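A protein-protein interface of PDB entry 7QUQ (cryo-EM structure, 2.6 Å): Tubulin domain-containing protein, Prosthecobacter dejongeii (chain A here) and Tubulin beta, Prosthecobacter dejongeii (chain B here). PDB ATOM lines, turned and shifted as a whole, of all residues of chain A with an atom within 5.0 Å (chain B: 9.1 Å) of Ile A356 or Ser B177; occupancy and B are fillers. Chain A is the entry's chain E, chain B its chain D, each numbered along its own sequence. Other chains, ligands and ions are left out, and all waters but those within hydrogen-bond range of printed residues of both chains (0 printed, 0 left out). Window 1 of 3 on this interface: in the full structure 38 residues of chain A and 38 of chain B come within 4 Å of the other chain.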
ATOM      1  N   VAL A 252     -12.894 -18.201   8.843  1.00  0.00           N
ATOM      2  CA  VAL A 252     -12.880 -17.283   7.714  1.00  0.00           C
ATOM      3  C   VAL A 252     -12.871 -18.119   6.441  1.00  0.00           C
ATOM      4  O   VAL A 252     -12.004 -18.983   6.256  1.00  0.00           O
ATOM      5  CB  VAL A 252     -11.698 -16.292   7.784  1.00  0.00           C
ATOM      6  CG1 VAL A 252     -11.825 -15.429   9.027  1.00  0.00           C
ATOM      7  CG2 VAL A 252     -10.356 -17.010   7.830  1.00  0.00           C
ATOM      8  N   VAL A 321      -1.922 -20.393   6.062  1.00  0.00           N
ATOM      9  CA  VAL A 321      -1.882 -21.375   7.138  1.00  0.00           C
ATOM     10  C   VAL A 321      -3.321 -21.622   7.558  1.00  0.00           C
ATOM     11  O   VAL A 321      -3.958 -20.751   8.157  1.00  0.00           O
ATOM     12  CB  VAL A 321      -1.025 -20.896   8.315  1.00  0.00           C
ATOM     13  CG1 VAL A 321      -1.129 -21.869   9.476  1.00  0.00           C
ATOM     14  CG2 VAL A 321       0.421 -20.728   7.880  1.00  0.00           C
ATOM     15  N   ASP A 334      -2.211 -17.743  17.795  1.00  0.00           N
ATOM     16  CA  ASP A 334      -1.811 -16.576  17.015  1.00  0.00           C
ATOM     17  C   ASP A 334      -0.439 -16.073  17.446  1.00  0.00           C
ATOM     18  O   ASP A 334       0.385 -15.692  16.605  1.00  0.00           O
ATOM     19  CB  ASP A 334      -2.857 -15.471  17.153  1.00  0.00           C
ATOM     20  CG  ASP A 334      -4.083 -15.720  16.298  1.00  0.00           C
ATOM     21  OD1 ASP A 334      -4.123 -16.760  15.608  1.00  0.00           O
ATOM     22  OD2 ASP A 334      -5.007 -14.881  16.320  1.00  0.00           O
ATOM     23  N   LEU A 337       2.117 -18.446  15.989  1.00  0.00           N
ATOM     24  CA  LEU A 337       2.332 -18.151  14.575  1.00  0.00           C
ATOM     25  C   LEU A 337       3.186 -16.901  14.393  1.00  0.00           C
ATOM     26  O   LEU A 337       4.088 -16.871  13.548  1.00  0.00           O
ATOM     27  CB  LEU A 337       0.992 -17.999  13.858  1.00  0.00           C
ATOM     28  CG  LEU A 337       0.155 -19.275  13.753  1.00  0.00           C
ATOM     29  CD1 LEU A 337      -1.216 -18.981  13.170  1.00  0.00           C
ATOM     30  CD2 LEU A 337       0.880 -20.315  12.916  1.00  0.00           C
ATOM     31  N   THR A 352       2.906  -8.738   4.968  1.00  0.00           N
ATOM     32  CA  THR A 352       1.675  -9.391   5.407  1.00  0.00           C
ATOM     33  C   THR A 352       1.510 -10.783   4.792  1.00  0.00           C
ATOM     34  O   THR A 352       0.445 -11.166   4.316  1.00  0.00           O
ATOM     35  CB  THR A 352       0.494  -8.483   5.075  1.00  0.00           C
ATOM     36  OG1 THR A 352      -0.726  -9.041   5.573  1.00  0.00           O
ATOM     37  CG2 THR A 352       0.393  -8.234   3.584  1.00  0.00           C
ATOM     38  N   ALA A 353       2.555 -11.600   4.882  1.00  0.00           N
ATOM     39  CA  ALA A 353       2.628 -12.832   4.106  1.00  0.00           C
ATOM     40  C   ALA A 353       1.888 -14.001   4.741  1.00  0.00           C
ATOM     41  O   ALA A 353       2.123 -15.146   4.337  1.00  0.00           O
ATOM     42  CB  ALA A 353       4.089 -13.211   3.865  1.00  0.00           C
ATOM     43  N   PHE A 354       1.008 -13.763   5.710  1.00  0.00           N
ATOM     44  CA  PHE A 354       0.275 -14.838   6.370  1.00  0.00           C
ATOM     45  C   PHE A 354      -1.220 -14.609   6.212  1.00  0.00           C
ATOM     46  O   PHE A 354      -1.743 -13.573   6.634  1.00  0.00           O
ATOM     47  CB  PHE A 354       0.654 -14.942   7.847  1.00  0.00           C
ATOM     48  CG  PHE A 354       1.842 -15.818   8.104  1.00  0.00           C
ATOM     49  CD1 PHE A 354       3.120 -15.385   7.797  1.00  0.00           C
ATOM     50  CD2 PHE A 354       1.679 -17.082   8.643  1.00  0.00           C
ATOM     51  CE1 PHE A 354       4.214 -16.194   8.031  1.00  0.00           C
ATOM     52  CE2 PHE A 354       2.767 -17.896   8.878  1.00  0.00           C
ATOM     53  CZ  PHE A 354       4.038 -17.452   8.571  1.00  0.00           C
ATOM     54  N   LYS A 355      -1.898 -15.569   5.591  1.00  0.00           N
ATOM     55  CA  LYS A 355      -3.349 -15.682   5.656  1.00  0.00           C
ATOM     56  C   LYS A 355      -3.668 -16.803   6.636  1.00  0.00           C
ATOM     57  O   LYS A 355      -3.538 -17.984   6.301  1.00  0.00           O
ATOM     58  CB  LYS A 355      -3.951 -15.963   4.281  1.00  0.00           C
ATOM     59  CG  LYS A 355      -5.467 -15.984   4.293  1.00  0.00           C
ATOM     60  CD  LYS A 355      -6.047 -15.947   2.902  1.00  0.00           C
ATOM     61  CE  LYS A 355      -7.514 -15.568   2.947  1.00  0.00           C
ATOM     62  NZ  LYS A 355      -7.725 -14.258   3.621  1.00  0.00           N
ATOM     63  N   ILE A 356      -4.067 -16.434   7.852  1.00  0.00           N
ATOM     64  CA  ILE A 356      -4.328 -17.413   8.905  1.00  0.00           C
ATOM     65  C   ILE A 356      -5.805 -17.790   8.803  1.00  0.00           C
ATOM     66  O   ILE A 356      -6.679 -17.204   9.443  1.00  0.00           O
ATOM     67  CB  ILE A 356      -3.927 -16.896  10.288  1.00  0.00           C
ATOM     68  CG1 ILE A 356      -4.432 -15.472  10.530  1.00  0.00           C
ATOM     69  CG2 ILE A 356      -2.416 -16.925  10.433  1.00  0.00           C
ATOM     70  CD1 ILE A 356      -4.033 -14.898  11.875  1.00  0.00           C
ATOM     71  N   GLY A 357      -6.081 -18.797   7.978  1.00  0.00           N
ATOM     72  CA  GLY A 357      -7.443 -19.261   7.802  1.00  0.00           C
ATOM     73  C   GLY A 357      -7.816 -20.232   8.904  1.00  0.00           C
ATOM     74  O   GLY A 357      -6.994 -21.047   9.337  1.00  0.00           O
ATOM     75  N   TYR A 358      -9.054 -20.137   9.370  1.00  0.00           N
ATOM     76  CA  TYR A 358      -9.571 -21.028  10.394  1.00  0.00           C
ATOM     77  C   TYR A 358     -10.782 -21.777   9.860  1.00  0.00           C
ATOM     78  O   TYR A 358     -11.515 -21.264   9.010  1.00  0.00           O
ATOM     79  CB  TYR A 358      -9.944 -20.265  11.672  1.00  0.00           C
ATOM     80  CG  TYR A 358     -10.573 -21.152  12.717  1.00  0.00           C
ATOM     81  CD1 TYR A 358      -9.814 -22.074  13.419  1.00  0.00           C
ATOM     82  CD2 TYR A 358     -11.930 -21.078  12.992  1.00  0.00           C
ATOM     83  CE1 TYR A 358     -10.390 -22.894  14.362  1.00  0.00           C
ATOM     84  CE2 TYR A 358     -12.513 -21.892  13.936  1.00  0.00           C
ATOM     85  CZ  TYR A 358     -11.739 -22.797  14.621  1.00  0.00           C
ATOM     86  OH  TYR A 358     -12.320 -23.610  15.565  1.00  0.00           O
ATOM     87  N   GLN B  11     -17.228 -10.092   6.690  1.00  0.00           N
ATOM     88  CA  GLN B  11     -17.405 -11.103   7.730  1.00  0.00           C
ATOM     89  C   GLN B  11     -17.113 -10.533   9.112  1.00  0.00           C
ATOM     90  O   GLN B  11     -17.857 -10.783  10.068  1.00  0.00           O
ATOM     91  CB  GLN B  11     -16.509 -12.309   7.448  1.00  0.00           C
ATOM     92  CG  GLN B  11     -16.251 -13.179   8.667  1.00  0.00           C
ATOM     93  CD  GLN B  11     -15.423 -14.403   8.346  1.00  0.00           C
ATOM     94  OE1 GLN B  11     -14.977 -14.590   7.214  1.00  0.00           O
ATOM     95  NE2 GLN B  11     -15.211 -15.248   9.347  1.00  0.00           N
ATOM     96  N   ASN B 100     -10.021 -10.858  -1.602  1.00  0.00           N
ATOM     97  CA  ASN B 100      -9.601  -9.815  -0.674  1.00  0.00           C
ATOM     98  C   ASN B 100      -9.266  -8.534  -1.424  1.00  0.00           C
ATOM     99  O   ASN B 100      -8.531  -7.686  -0.920  1.00  0.00           O
ATOM    100  CB  ASN B 100      -8.412 -10.256   0.180  1.00  0.00           C
ATOM    101  CG  ASN B 100      -8.766 -11.359   1.157  1.00  0.00           C
ATOM    102  OD1 ASN B 100      -8.230 -12.462   1.083  1.00  0.00           O
ATOM    103  ND2 ASN B 100      -9.672 -11.063   2.080  1.00  0.00           N
ATOM    104  N   GLY B 141      -9.182  -4.469   6.397  1.00  0.00           N
ATOM    105  CA  GLY B 141      -8.256  -5.427   5.836  1.00  0.00           C
ATOM    106  C   GLY B 141      -8.851  -6.487   4.938  1.00  0.00           C
ATOM    107  O   GLY B 141      -8.101  -7.246   4.317  1.00  0.00           O
ATOM    108  N   VAL B 171      -8.914  -2.627  12.371  1.00  0.00           N
ATOM    109  CA  VAL B 171      -7.634  -2.537  11.681  1.00  0.00           C
ATOM    110  C   VAL B 171      -6.938  -3.886  11.827  1.00  0.00           C
ATOM    111  O   VAL B 171      -7.055  -4.524  12.885  1.00  0.00           O
ATOM    112  CB  VAL B 171      -6.784  -1.385  12.240  1.00  0.00           C
ATOM    113  CG1 VAL B 171      -5.450  -1.294  11.517  1.00  0.00           C
ATOM    114  CG2 VAL B 171      -7.543  -0.070  12.139  1.00  0.00           C
ATOM    115  N   PRO B 172      -6.237  -4.370  10.803  1.00  0.00           N
ATOM    116  CA  PRO B 172      -5.503  -5.634  10.938  1.00  0.00           C
ATOM    117  C   PRO B 172      -4.455  -5.592  12.041  1.00  0.00           C
ATOM    118  O   PRO B 172      -3.894  -4.542  12.360  1.00  0.00           O
ATOM    119  CB  PRO B 172      -4.849  -5.814   9.563  1.00  0.00           C
ATOM    120  CG  PRO B 172      -5.139  -4.552   8.788  1.00  0.00           C
ATOM    121  CD  PRO B 172      -6.361  -3.966   9.394  1.00  0.00           C
ATOM    122  N   SER B 173      -4.203  -6.764  12.623  1.00  0.00           N
ATOM    123  CA  SER B 173      -3.310  -6.878  13.764  1.00  0.00           C
ATOM    124  C   SER B 173      -1.866  -6.575  13.366  1.00  0.00           C
ATOM    125  O   SER B 173      -1.462  -6.822  12.228  1.00  0.00           O
ATOM    126  CB  SER B 173      -3.382  -8.282  14.355  1.00  0.00           C
ATOM    127  OG  SER B 173      -4.710  -8.633  14.679  1.00  0.00           O
ATOM    128  N   PRO B 174      -1.070  -6.037  14.291  1.00  0.00           N
ATOM    129  CA  PRO B 174       0.351  -5.809  14.001  1.00  0.00           C
ATOM    130  C   PRO B 174       1.193  -7.074  14.080  1.00  0.00           C
ATOM    131  O   PRO B 174       2.119  -7.255  13.284  1.00  0.00           O
ATOM    132  CB  PRO B 174       0.773  -4.798  15.079  1.00  0.00           C
ATOM    133  CG  PRO B 174      -0.514  -4.270  15.660  1.00  0.00           C
ATOM    134  CD  PRO B 174      -1.477  -5.401  15.553  1.00  0.00           C
ATOM    135  N   LEU B 175       0.884  -7.959  15.034  1.00  0.00           N
ATOM    136  CA  LEU B 175       1.756  -9.101  15.294  1.00  0.00           C
ATOM    137  C   LEU B 175       1.625 -10.184  14.232  1.00  0.00           C
ATOM    138  O   LEU B 175       2.614 -10.850  13.906  1.00  0.00           O
ATOM    139  CB  LEU B 175       1.473  -9.702  16.675  1.00  0.00           C
ATOM    140  CG  LEU B 175       0.229 -10.575  16.906  1.00  0.00           C
ATOM    141  CD1 LEU B 175       0.345 -11.338  18.219  1.00  0.00           C
ATOM    142  CD2 LEU B 175      -1.066  -9.785  16.852  1.00  0.00           C
ATOM    143  N   ILE B 176       0.426 -10.379  13.685  1.00  0.00           N
ATOM    144  CA  ILE B 176       0.191 -11.422  12.696  1.00  0.00           C
ATOM    145  C   ILE B 176      -0.948 -10.961  11.802  1.00  0.00           C
ATOM    146  O   ILE B 176      -1.874 -10.280  12.251  1.00  0.00           O
ATOM    147  CB  ILE B 176      -0.106 -12.787  13.372  1.00  0.00           C
ATOM    148  CG1 ILE B 176      -0.159 -13.912  12.333  1.00  0.00           C
ATOM    149  CG2 ILE B 176      -1.389 -12.731  14.192  1.00  0.00           C
ATOM    150  CD1 ILE B 176       1.160 -14.169  11.642  1.00  0.00           C
ATOM    151  N   SER B 177      -0.864 -11.315  10.526  1.00  0.00           N
ATOM    152  CA  SER B 177      -1.825 -10.890   9.523  1.00  0.00           C
ATOM    153  C   SER B 177      -2.762 -12.035   9.177  1.00  0.00           C
ATOM    154  O   SER B 177      -2.446 -13.204   9.416  1.00  0.00           O
ATOM    155  CB  SER B 177      -1.107 -10.411   8.268  1.00  0.00           C
ATOM    156  OG  SER B 177      -0.398 -11.470   7.649  1.00  0.00           O
ATOM    157  N   ASP B 178      -3.920 -11.694   8.609  1.00  0.00           N
ATOM    158  CA  ASP B 178      -4.855 -12.727   8.186  1.00  0.00           C
ATOM    159  C   ASP B 178      -5.139 -12.592   6.689  1.00  0.00           C
ATOM    160  O   ASP B 178      -5.769 -13.463   6.086  1.00  0.00           O
ATOM    161  CB  ASP B 178      -6.132 -12.629   9.031  1.00  0.00           C
ATOM    162  CG  ASP B 178      -7.093 -13.808   8.842  1.00  0.00           C
ATOM    163  OD1 ASP B 178      -6.834 -14.729   8.041  1.00  0.00           O
ATOM    164  OD2 ASP B 178      -8.131 -13.818   9.532  1.00  0.00           O
ATOM    165  N   SER B 179      -4.674 -11.514   6.065  1.00  0.00           N
ATOM    166  CA  SER B 179      -4.770 -11.362   4.622  1.00  0.00           C
ATOM    167  C   SER B 179      -3.428 -10.917   4.056  1.00  0.00           C
ATOM    168  O   SER B 179      -2.657 -10.215   4.716  1.00  0.00           O
ATOM    169  CB  SER B 179      -5.860 -10.358   4.229  1.00  0.00           C
ATOM    170  OG  SER B 179      -5.950 -10.234   2.820  1.00  0.00           O
ATOM    171  N   ALA B 180      -3.155 -11.343   2.821  1.00  0.00           N
ATOM    172  CA  ALA B 180      -1.872 -11.044   2.194  1.00  0.00           C
ATOM    173  C   ALA B 180      -1.912  -9.774   1.356  1.00  0.00           C
ATOM    174  O   ALA B 180      -0.870  -9.332   0.860  1.00  0.00           O
ATOM    175  CB  ALA B 180      -1.420 -12.224   1.337  1.00  0.00           C
ATOM    176  N   VAL B 181      -3.098  -9.191   1.163  1.00  0.00           N
ATOM    177  CA  VAL B 181      -3.222  -7.935   0.432  1.00  0.00           C
ATOM    178  C   VAL B 181      -3.899  -6.863   1.279  1.00  0.00           C
ATOM    179  O   VAL B 181      -4.284  -5.807   0.758  1.00  0.00           O
ATOM    180  CB  VAL B 181      -3.954  -8.217  -0.901  1.00  0.00           C
ATOM    181  CG1 VAL B 181      -5.434  -8.423  -0.673  1.00  0.00           C
ATOM    182  CG2 VAL B 181      -3.677  -7.136  -1.943  1.00  0.00           C
ATOM    183  N   GLU B 182      -4.010  -7.084   2.585  1.00  0.00           N
ATOM    184  CA  GLU B 182      -4.732  -6.229   3.520  1.00  0.00           C
ATOM    185  C   GLU B 182      -4.175  -4.815   3.726  1.00  0.00           C
ATOM    186  O   GLU B 182      -4.957  -3.940   4.111  1.00  0.00           O
ATOM    187  CB  GLU B 182      -4.859  -6.957   4.864  1.00  0.00           C
ATOM    188  CG  GLU B 182      -3.725  -6.767   5.843  1.00  0.00           C
ATOM    189  CD  GLU B 182      -3.841  -7.684   7.034  1.00  0.00           C
ATOM    190  OE1 GLU B 182      -4.909  -8.309   7.200  1.00  0.00           O
ATOM    191  OE2 GLU B 182      -2.872  -7.769   7.815  1.00  0.00           O
ATOM    192  N   PRO B 183      -2.879  -4.515   3.529  1.00  0.00           N
ATOM    193  CA  PRO B 183      -2.484  -3.097   3.591  1.00  0.00           C
ATOM    194  C   PRO B 183      -3.069  -2.265   2.466  1.00  0.00           C
ATOM    195  O   PRO B 183      -3.500  -1.131   2.718  1.00  0.00           O
ATOM    196  CB  PRO B 183      -0.952  -3.144   3.514  1.00  0.00           C
ATOM    197  CG  PRO B 183      -0.596  -4.489   3.953  1.00  0.00           C
ATOM    198  CD  PRO B 183      -1.681  -5.370   3.443  1.00  0.00           C
ATOM    199  N   ASN B 205      -7.241  -6.006  16.886  1.00  0.00           N
ATOM    200  CA  ASN B 205      -7.591  -7.341  17.358  1.00  0.00           C
ATOM    201  C   ASN B 205      -6.787  -7.745  18.588  1.00  0.00           C
ATOM    202  O   ASN B 205      -7.366  -8.200  19.577  1.00  0.00           O
ATOM    203  CB  ASN B 205      -7.385  -8.364  16.247  1.00  0.00           C
ATOM    204  CG  ASN B 205      -8.654  -8.671  15.490  1.00  0.00           C
ATOM    205  OD1 ASN B 205      -9.747  -8.230  15.860  1.00  0.00           O
ATOM    206  ND2 ASN B 205      -8.517  -9.439  14.415  1.00  0.00           N
ATOM    207  N   PHE B 209      -7.674  -9.164  22.244  1.00  0.00           N
ATOM    208  CA  PHE B 209      -7.262 -10.453  22.796  1.00  0.00           C
ATOM    209  C   PHE B 209      -6.694 -10.295  24.199  1.00  0.00           C
ATOM    210  O   PHE B 209      -7.029 -11.068  25.099  1.00  0.00           O
ATOM    211  CB  PHE B 209      -6.235 -11.159  21.902  1.00  0.00           C
ATOM    212  CG  PHE B 209      -6.779 -11.674  20.596  1.00  0.00           C
ATOM    213  CD1 PHE B 209      -7.530 -12.836  20.562  1.00  0.00           C
ATOM    214  CD2 PHE B 209      -6.450 -11.070  19.398  1.00  0.00           C
ATOM    215  CE1 PHE B 209      -8.006 -13.338  19.366  1.00  0.00           C
ATOM    216  CE2 PHE B 209      -6.920 -11.566  18.199  1.00  0.00           C
ATOM    217  CZ  PHE B 209      -7.693 -12.706  18.182  1.00  0.00           C
ATOM    218  N   TYR B 222     -12.817 -14.611  18.758  1.00  0.00           N
ATOM    219  CA  TYR B 222     -13.452 -13.431  18.166  1.00  0.00           C
ATOM    220  C   TYR B 222     -14.803 -13.106  18.789  1.00  0.00           C
ATOM    221  O   TYR B 222     -15.217 -11.942  18.762  1.00  0.00           O
ATOM    222  CB  TYR B 222     -13.620 -13.592  16.652  1.00  0.00           C
ATOM    223  CG  TYR B 222     -12.342 -13.575  15.844  1.00  0.00           C
ATOM    224  CD1 TYR B 222     -11.152 -13.124  16.396  1.00  0.00           C
ATOM    225  CD2 TYR B 222     -12.336 -13.979  14.516  1.00  0.00           C
ATOM    226  CE1 TYR B 222      -9.989 -13.088  15.651  1.00  0.00           C
ATOM    227  CE2 TYR B 222     -11.177 -13.950  13.766  1.00  0.00           C
ATOM    228  CZ  TYR B 222     -10.006 -13.504  14.340  1.00  0.00           C
ATOM    229  OH  TYR B 222      -8.847 -13.474  13.598  1.00  0.00           O
ATOM    230  N   LEU B 381       0.284   0.339   8.589  1.00  0.00           N
ATOM    231  CA  LEU B 381      -0.217  -0.046   7.277  1.00  0.00           C
ATOM    232  C   LEU B 381       0.602   0.630   6.193  1.00  0.00           C
ATOM    233  O   LEU B 381       1.109  -0.035   5.278  1.00  0.00           O
ATOM    234  CB  LEU B 381      -1.697   0.316   7.149  1.00  0.00           C
ATOM    235  CG  LEU B 381      -2.611  -0.240   8.241  1.00  0.00           C
ATOM    236  CD1 LEU B 381      -3.916   0.537   8.303  1.00  0.00           C
ATOM    237  CD2 LEU B 381      -2.874  -1.717   8.016  1.00  0.00           C
ATOM    238  N   GLN B 384       3.874  -1.088   5.828  1.00  0.00           N
ATOM    239  CA  GLN B 384       3.757  -2.258   4.972  1.00  0.00           C
ATOM    240  C   GLN B 384       3.553  -1.839   3.525  1.00  0.00           C
ATOM    241  O   GLN B 384       4.214  -2.376   2.625  1.00  0.00           O
ATOM    242  CB  GLN B 384       2.621  -3.150   5.471  1.00  0.00           C
ATOM    243  CG  GLN B 384       2.929  -3.774   6.828  1.00  0.00           C
ATOM    244  CD  GLN B 384       1.750  -4.503   7.442  1.00  0.00           C
ATOM    245  OE1 GLN B 384       0.850  -4.958   6.740  1.00  0.00           O
ATOM    246  NE2 GLN B 384       1.757  -4.622   8.763  1.00  0.00           N
ATOM    247  N   MET B 388       5.336  -2.844   0.051  1.00  0.00           N
ATOM    248  CA  MET B 388       4.463  -3.624  -0.816  1.00  0.00           C
ATOM    249  C   MET B 388       4.285  -2.965  -2.179  1.00  0.00           C
ATOM    250  O   MET B 388       4.403  -3.632  -3.213  1.00  0.00           O
ATOM    251  CB  MET B 388       3.115  -3.813  -0.127  1.00  0.00           C
ATOM    252  CG  MET B 388       2.103  -4.593  -0.918  1.00  0.00           C
ATOM    253  SD  MET B 388       0.811  -5.244   0.144  1.00  0.00           S
ATOM    254  CE  MET B 388       1.811  -5.734   1.537  1.00  0.00           C
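The side-chain hydroxyl of Ser B177 sits close to the side-chain hydroxyl of Thr A352, 3.2 Å away.
The backbone carbonyl oxygen (O) of Ser B179 lies within hydrogen-bond range of the side-chain hydroxyl (OG1) of Thr A352 (2.4 Å).
The side-chain carboxylate (OE2) of Glu B182 sits at hydrogen-bond distance from the side-chain hydroxyl (OG1) of Thr A352, at 3.4 Å.
OG of Ser B177 is in hydrogen-bond range of O of Phe A354.
The backbone NH (N) of Asp B178 lies within hydrogen-bond range of the backbone carbonyl oxygen (O) of Phe A354 (3.5 Å).
The side-chain amide oxygen (OD1) of Asn B100 sits at hydrogen-bond distance from the side-chain amino group (NZ) of Lys A355 (3.1 Å).
O of Asp B178 sits close to NZ of Lys A355, 3.2 Å away.
The backbone NH (N) of Ile A356 lies within hydrogen-bond range of the side-chain carboxylate (OD1) of Asp B178 (3.3 Å).
The backbone carbonyl oxygen (O) of Tyr A358 sits at hydrogen-bond distance from the backbone NH (N) of Val A252, 3.4 Å away.
The backbone carbonyl oxygen (O) of Lys A355 sits at hydrogen-bond distance from the backbone NH (N) of Val A321, 2.9 Å away.
The side-chain hydroxyl (OG) of Ser B179 sits close to the backbone NH (N) of Val B181 (3.5 Å).
N of Ser B179 is in hydrogen-bond range of OE1 of Glu B182, at 3.4 Å.
Gln B11 touches Val A252.
Asp A334 touches Phe B209 (OD2 to CZ, 3.9 Å).
Thr A352 touches Ala B180.
Thr A352 touches Pro B183.
Gln B384 touches Thr A352.
Thr A352 touches Met B388.
Phe A354 touches Ile B176.
O of Phe A354 touches N of Ser B179, 3.6 Å away.
Ile A356 touches Ser B177 (CG1 to O, 3.2 Å).
Leu A337 touches none of the printed residues of chain B.
Of chain B, only Ser B177 and Asp B178 come within 4 Å of Ile A356.
Of the printed residues of chain A, Gln B11 touches Val A252.
Printed residues of chain A within 4 Å of Asn B100: Lys A355 (3.1 Å).
Printed residues of chain A within 4 Å of Ile B176: Phe A354 (3.9 Å).
Of chain A, only Thr A352 (3.0 Å), Phe A354 (2.7 Å) and Ile A356 (3.2 Å) come within 4 Å of Ser B177.
Of the printed residues of chain A, Glu B182 touches Thr A352 (3.4 Å).
Printed residues of chain A within 4 Å of Phe B209: Asp A334.
The nearest residue of chain A that does not touch Ser B177 is Ala A353 (4.05 Å).
Of the 22 printed residues of chain B, 12 touch a printed residue of chain A.
Printed residues of chain A that touch a printed residue of chain B: Val A252, Asp A334, Thr A352, Phe A354, Lys A355 and Ile A356.
Hydrophobic or aromatic side chains of chain A that line the printed part of chain B: Val A252, Phe A354 and Ile A356.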
